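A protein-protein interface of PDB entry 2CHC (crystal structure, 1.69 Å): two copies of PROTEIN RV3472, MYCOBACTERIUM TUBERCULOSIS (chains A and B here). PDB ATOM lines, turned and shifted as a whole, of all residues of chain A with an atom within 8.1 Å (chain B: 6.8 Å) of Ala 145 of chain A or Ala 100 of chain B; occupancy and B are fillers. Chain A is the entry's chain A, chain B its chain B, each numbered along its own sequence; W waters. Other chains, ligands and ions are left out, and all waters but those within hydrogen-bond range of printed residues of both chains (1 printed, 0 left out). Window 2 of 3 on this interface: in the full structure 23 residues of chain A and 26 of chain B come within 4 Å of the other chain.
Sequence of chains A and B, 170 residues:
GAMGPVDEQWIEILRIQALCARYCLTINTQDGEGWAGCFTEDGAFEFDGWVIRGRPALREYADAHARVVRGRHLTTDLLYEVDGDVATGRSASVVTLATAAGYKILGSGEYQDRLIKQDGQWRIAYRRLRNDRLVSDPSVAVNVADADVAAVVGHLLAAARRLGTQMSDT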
ATOM      1  N   LEU A 106      -8.967  -5.469   4.829  1.00  0.00           N
ATOM      2  CA  LEU A 106      -9.257  -5.152   6.190  1.00  0.00           C
ATOM      3  C   LEU A 106     -10.383  -5.988   6.741  1.00  0.00           C
ATOM      4  O   LEU A 106     -10.381  -6.420   7.910  1.00  0.00           O
ATOM      5  CB  LEU A 106      -9.592  -3.671   6.325  1.00  0.00           C
ATOM      6  CG  LEU A 106     -10.110  -3.112   7.653  1.00  0.00           C
ATOM      7  CD1 LEU A 106      -9.068  -3.304   8.732  1.00  0.00           C
ATOM      8  CD2 LEU A 106     -10.454  -1.653   7.475  1.00  0.00           C
ATOM      9  N   LEU A 134     -12.225 -17.374  11.570  1.00  0.00           N
ATOM     10  CA  LEU A 134     -11.533 -18.638  11.346  1.00  0.00           C
ATOM     11  C   LEU A 134     -12.443 -19.817  11.667  1.00  0.00           C
ATOM     12  O   LEU A 134     -13.039 -19.872  12.755  1.00  0.00           O
ATOM     13  CB  LEU A 134     -10.263 -18.738  12.204  1.00  0.00           C
ATOM     14  CG  LEU A 134      -8.959 -18.437  11.472  1.00  0.00           C
ATOM     15  CD1 LEU A 134      -8.994 -17.017  11.047  1.00  0.00           C
ATOM     16  CD2 LEU A 134      -7.754 -18.662  12.331  1.00  0.00           C
ATOM     17  N   SER A 136     -11.494 -22.748  12.289  1.00  0.00           N
ATOM     18  CA  SER A 136     -10.831 -23.562  13.308  1.00  0.00           C
ATOM     19  C   SER A 136     -10.804 -22.919  14.695  1.00  0.00           C
ATOM     20  O   SER A 136     -10.745 -23.631  15.708  1.00  0.00           O
ATOM     21  CB  SER A 136      -9.393 -23.853  12.875  1.00  0.00           C
ATOM     22  OG  SER A 136      -8.616 -22.665  12.868  1.00  0.00           O
ATOM     23  N   VAL A 140     -10.763 -16.061  17.567  1.00  0.00           N
ATOM     24  CA  VAL A 140      -9.860 -15.118  16.905  1.00  0.00           C
ATOM     25  C   VAL A 140     -10.547 -14.160  15.910  1.00  0.00           C
ATOM     26  O   VAL A 140     -11.255 -14.592  14.981  1.00  0.00           O
ATOM     27  N   ALA A 141     -10.338 -12.860  16.127  1.00  0.00           N
ATOM     28  CA  ALA A 141     -10.688 -11.838  15.145  1.00  0.00           C
ATOM     29  C   ALA A 141      -9.611 -11.856  14.067  1.00  0.00           C
ATOM     30  O   ALA A 141      -8.426 -11.681  14.364  1.00  0.00           O
ATOM     31  CB  ALA A 141     -10.770 -10.470  15.790  1.00  0.00           C
ATOM     32  N   VAL A 142     -10.025 -12.066  12.821  1.00  0.00           N
ATOM     33  CA  VAL A 142      -9.083 -12.271  11.709  1.00  0.00           C
ATOM     34  C   VAL A 142      -8.468 -10.954  11.255  1.00  0.00           C
ATOM     35  O   VAL A 142      -7.360 -10.941  10.708  1.00  0.00           O
ATOM     36  CB  VAL A 142      -9.776 -12.935  10.518  1.00  0.00           C
ATOM     37  CG1 VAL A 142      -8.756 -13.304   9.425  1.00  0.00           C
ATOM     38  CG2 VAL A 142     -10.561 -14.149  11.001  1.00  0.00           C
ATOM     39  N   ASN A 143      -9.193  -9.857  11.503  1.00  0.00           N
ATOM     40  CA  ASN A 143      -8.705  -8.509  11.225  1.00  0.00           C
ATOM     41  C   ASN A 143      -7.393  -8.192  11.967  1.00  0.00           C
ATOM     42  O   ASN A 143      -6.517  -7.516  11.426  1.00  0.00           O
ATOM     43  N   VAL A 144      -7.248  -8.709  13.182  1.00  0.00           N
ATOM     44  CA  VAL A 144      -6.057  -8.440  13.985  1.00  0.00           C
ATOM     45  C   VAL A 144      -4.816  -9.260  13.611  1.00  0.00           C
ATOM     46  O   VAL A 144      -3.784  -9.146  14.287  1.00  0.00           O
ATOM     47  N   ALA A 145      -4.902 -10.074  12.553  1.00  0.00           N
ATOM     48  CA  ALA A 145      -3.800 -10.963  12.168  1.00  0.00           C
ATOM     49  C   ALA A 145      -2.610 -10.227  11.517  1.00  0.00           C
ATOM     50  O   ALA A 145      -1.459 -10.540  11.838  1.00  0.00           O
ATOM     51  CB  ALA A 145      -4.303 -12.098  11.262  1.00  0.00           C
ATOM     52  N   ASP A 146      -2.873  -9.279  10.607  1.00  0.00           N
ATOM     53  CA  ASP A 146      -1.792  -8.482   9.977  1.00  0.00           C
ATOM     54  C   ASP A 146      -1.581  -7.168  10.756  1.00  0.00           C
ATOM     55  O   ASP A 146      -2.549  -6.535  11.119  1.00  0.00           O
ATOM     56  CB  ASP A 146      -2.133  -8.211   8.503  1.00  0.00           C
ATOM     57  CG  ASP A 146      -1.145  -7.265   7.830  1.00  0.00           C
ATOM     58  OD1 ASP A 146      -0.897  -6.159   8.373  1.00  0.00           O
ATOM     59  OD2 ASP A 146      -0.633  -7.617   6.742  1.00  0.00           O
ATOM     60  N   ALA A 147      -0.332  -6.747  10.983  1.00  0.00           N
ATOM     61  CA  ALA A 147      -0.051  -5.658  11.967  1.00  0.00           C
ATOM     62  C   ALA A 147      -0.473  -4.213  11.606  1.00  0.00           C
ATOM     63  O   ALA A 147      -0.929  -3.446  12.473  1.00  0.00           O
ATOM     64  CB  ALA A 147       1.423  -5.675  12.355  1.00  0.00           C
ATOM     65  N   ASP A 148      -0.268  -3.829  10.348  1.00  0.00           N
ATOM     66  CA  ASP A 148      -0.892  -2.624   9.761  1.00  0.00           C
ATOM     67  C   ASP A 148      -2.392  -2.645  10.005  1.00  0.00           C
ATOM     68  O   ASP A 148      -3.027  -1.698  10.569  1.00  0.00           O
ATOM     69  CB  ASP A 148      -0.698  -2.648   8.234  1.00  0.00           C
ATOM     70  N   VAL A 149      -2.966  -3.753   9.546  1.00  0.00           N
ATOM     71  CA  VAL A 149      -4.377  -3.940   9.652  1.00  0.00           C
ATOM     72  C   VAL A 149      -4.795  -3.885  11.093  1.00  0.00           C
ATOM     73  O   VAL A 149      -5.783  -3.243  11.412  1.00  0.00           O
ATOM     74  CB  VAL A 149      -4.810  -5.265   8.986  1.00  0.00           C
ATOM     75  CG1 VAL A 149      -6.218  -5.624   9.320  1.00  0.00           C
ATOM     76  CG2 VAL A 149      -4.645  -5.134   7.494  1.00  0.00           C
ATOM     77  N   ALA A 150      -4.025  -4.524  11.979  1.00  0.00           N
ATOM     78  CA  ALA A 150      -4.458  -4.718  13.346  1.00  0.00           C
ATOM     79  C   ALA A 150      -4.593  -3.395  14.083  1.00  0.00           C
ATOM     80  O   ALA A 150      -5.473  -3.251  14.895  1.00  0.00           O
ATOM     81  CB  ALA A 150      -3.492  -5.631  14.090  1.00  0.00           C
ATOM     82  N   ALA A 151      -3.741  -2.427  13.776  1.00  0.00           N
ATOM     83  CA  ALA A 151      -3.819  -1.139  14.475  1.00  0.00           C
ATOM     84  C   ALA A 151      -5.113  -0.422  14.083  1.00  0.00           C
ATOM     85  O   ALA A 151      -5.810   0.192  14.936  1.00  0.00           O
ATOM     86  CB  ALA A 151      -2.635  -0.307  14.117  1.00  0.00           C
ATOM     87  N   VAL A 153      -7.898  -1.809  13.049  1.00  0.00           N
ATOM     88  CA  VAL A 153      -8.955  -2.552  13.724  1.00  0.00           C
ATOM     89  C   VAL A 153      -9.118  -2.090  15.177  1.00  0.00           C
ATOM     90  O   VAL A 153     -10.237  -1.887  15.647  1.00  0.00           O
ATOM     91  CB  VAL A 153      -8.693  -4.070  13.625  1.00  0.00           C
ATOM     92  CG1 VAL A 153      -9.560  -4.876  14.622  1.00  0.00           C
ATOM     93  CG2 VAL A 153      -8.895  -4.524  12.180  1.00  0.00           C
ATOM     94  N   ALA B  98     -10.492 -16.131   5.253  1.00  0.00           N
ATOM     95  CA  ALA B  98      -9.947 -15.837   6.568  1.00  0.00           C
ATOM     96  C   ALA B  98      -8.823 -16.822   6.815  1.00  0.00           C
ATOM     97  O   ALA B  98      -9.048 -18.018   6.670  1.00  0.00           O
ATOM     98  CB  ALA B  98     -11.055 -16.031   7.660  1.00  0.00           C
ATOM     99  N   THR B  99      -7.629 -16.311   7.053  1.00  0.00           N
ATOM    100  CA  THR B  99      -6.469 -17.143   7.366  1.00  0.00           C
ATOM    101  C   THR B  99      -5.829 -16.675   8.631  1.00  0.00           C
ATOM    102  O   THR B  99      -6.139 -15.604   9.168  1.00  0.00           O
ATOM    103  CB  THR B  99      -5.385 -17.133   6.282  1.00  0.00           C
ATOM    104  OG1 THR B  99      -4.538 -15.995   6.443  1.00  0.00           O
ATOM    105  CG2 THR B  99      -5.953 -17.267   4.872  1.00  0.00           C
ATOM    106  N   ALA B 100      -4.889 -17.473   9.140  1.00  0.00           N
ATOM    107  CA  ALA B 100      -4.221 -17.079  10.371  1.00  0.00           C
ATOM    108  C   ALA B 100      -3.224 -15.951  10.115  1.00  0.00           C
ATOM    109  O   ALA B 100      -2.617 -15.419  11.033  1.00  0.00           O
ATOM    110  CB  ALA B 100      -3.513 -18.295  10.977  1.00  0.00           C
ATOM    111  N   ALA B 101      -3.037 -15.590   8.847  1.00  0.00           N
ATOM    112  CA  ALA B 101      -2.225 -14.454   8.500  1.00  0.00           C
ATOM    113  C   ALA B 101      -3.118 -13.297   7.987  1.00  0.00           C
ATOM    114  O   ALA B 101      -2.618 -12.396   7.344  1.00  0.00           O
ATOM    115  CB  ALA B 101      -1.300 -14.854   7.466  1.00  0.00           C
ATOM    116  N   GLY B 102      -4.407 -13.307   8.277  1.00  0.00           N
ATOM    117  CA  GLY B 102      -5.260 -12.211   7.806  1.00  0.00           C
ATOM    118  C   GLY B 102      -6.157 -12.662   6.694  1.00  0.00           C
ATOM    119  O   GLY B 102      -6.203 -13.816   6.326  1.00  0.00           O
ATOM    120  N   TYR B 103      -6.927 -11.729   6.153  1.00  0.00           N
ATOM    121  CA  TYR B 103      -7.748 -12.060   5.018  1.00  0.00           C
ATOM    122  C   TYR B 103      -6.885 -12.043   3.735  1.00  0.00           C
ATOM    123  O   TYR B 103      -5.999 -11.162   3.553  1.00  0.00           O
ATOM    124  CB  TYR B 103      -8.875 -11.049   4.883  1.00  0.00           C
ATOM    125  CG  TYR B 103      -9.881 -11.062   5.990  1.00  0.00           C
ATOM    126  CD1 TYR B 103     -10.768 -12.112   6.153  1.00  0.00           C
ATOM    127  CD2 TYR B 103     -10.015  -9.960   6.830  1.00  0.00           C
ATOM    128  CE1 TYR B 103     -11.705 -12.102   7.190  1.00  0.00           C
ATOM    129  CE2 TYR B 103     -10.959  -9.964   7.895  1.00  0.00           C
ATOM    130  CZ  TYR B 103     -11.821 -11.041   8.019  1.00  0.00           C
ATOM    131  OH  TYR B 103     -12.744 -11.099   9.068  1.00  0.00           O
ATOM    132  N   ASP B 148      -0.994 -20.202   2.741  1.00  0.00           N
ATOM    133  CA  ASP B 148      -2.218 -20.084   3.599  1.00  0.00           C
ATOM    134  C   ASP B 148      -3.453 -20.413   2.761  1.00  0.00           C
ATOM    135  O   ASP B 148      -4.376 -21.117   3.177  1.00  0.00           O
ATOM    136  CB  ASP B 148      -2.288 -18.673   4.226  1.00  0.00           C
ATOM    137  CG  ASP B 148      -1.180 -18.400   5.225  1.00  0.00           C
ATOM    138  OD1 ASP B 148      -0.412 -17.438   5.070  1.00  0.00           O
ATOM    139  OD2 ASP B 148      -1.083 -19.179   6.181  1.00  0.00           O
HETATM  140  O   HOH W   1     -12.107 -10.199  12.067  1.00  0.00           O
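N of Ala 101 of chain B lies within hydrogen-bond range of OG1 of Thr 99 of chain B (2.9 Å).
OG1 of Thr 99 of chain B lies within hydrogen-bond range of O of Gly 102 of chain B.
Tyr 103 of chain B touches Leu 106 of chain A (CE2 to O, 3.6 Å).
O of Thr 99 of chain B touches CD1 of Leu 134 of chain A (3.7 Å).
Val 142 of chain A touches Ala 98 of chain B (CG2 to CB, 3.9 Å).
Thr 99 of chain B touches Val 142 of chain A (O to CG1, 3.5 Å).
O of Val 142 of chain A touches CA of Gly 102 of chain B, at 3.8 Å.
Val 142 of chain A touches Tyr 103 of chain B.
Ala 145 of chain A touches Ala 100 of chain B (CB to O, 3.7 Å).
Ala 145 of chain A touches Ala 101 of chain B.
CB of Ala 145 of chain A touches N of Gly 102 of chain B, 3.2 Å away.
Of the 16 printed residues of chain A, 4 touch a printed residue of chain B.
Hydrophobic or aromatic side chains of chain A within 4 Å of the printed part of chain B: Leu 134, Val 142 and Ala 145.
Of the 7 printed residues of chain B, 6 touch a printed residue of chain A.
Printed residues of chain B that touch a printed residue of chain A: Ala 98, Thr 99, Ala 100, Ala 101, Gly 102 and Tyr 103.
Hydrophobic or aromatic side chains of chain B within 4 Å of the printed part of chain A: Ala 98 and Tyr 103.
Among the printed residues, no Asp or Glu carboxylate lies within 4 Å of a Lys or Arg side-chain nitrogen of the other chain.
Water W1 lies within hydrogen-bond range of N of Val 142 of chain A (2.9 Å), N of Asn 143 of chain A (3.0 Å) and OH of Tyr 103 of chain B (3.2 Å).
1 position is printed for both chains.
Of the 9 pairs that touch across the chains among the printed residues, none has its exchanged pair printed and touching as well.
Of chain B, only Ala 100, Ala 101 and Gly 102 come within 4 Å of Ala 145 of chain A.
Of the printed residues of chain A, Gly 102 of chain B touches Val 142 and Ala 145.
Of the printed residues of chain B, Val 142 of chain A touches Ala 98 (3.9 Å), Thr 99 (3.5 Å), Gly 102 (3.8 Å) and Tyr 103 (3.7 Å).
Of the printed residues of chain B, Leu 134 of chain A touches Thr 99 (3.7 Å).
Printed residues of chain A within 4 Å of Tyr 103 of chain B: Leu 106 (3.6 Å) and Val 142 (3.7 Å).
The nearest residue of chain B that does not touch Ala 145 of chain A is Thr 99 of chain B (4.5 Å).
The nearest residue of chain A that does not touch Ala 100 of chain B is Leu 134 of chain A (4.3 Å).
The nearest printed residue of chain A that does not touch Ala 98 of chain B is Leu 134 of chain A (4.1 Å).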
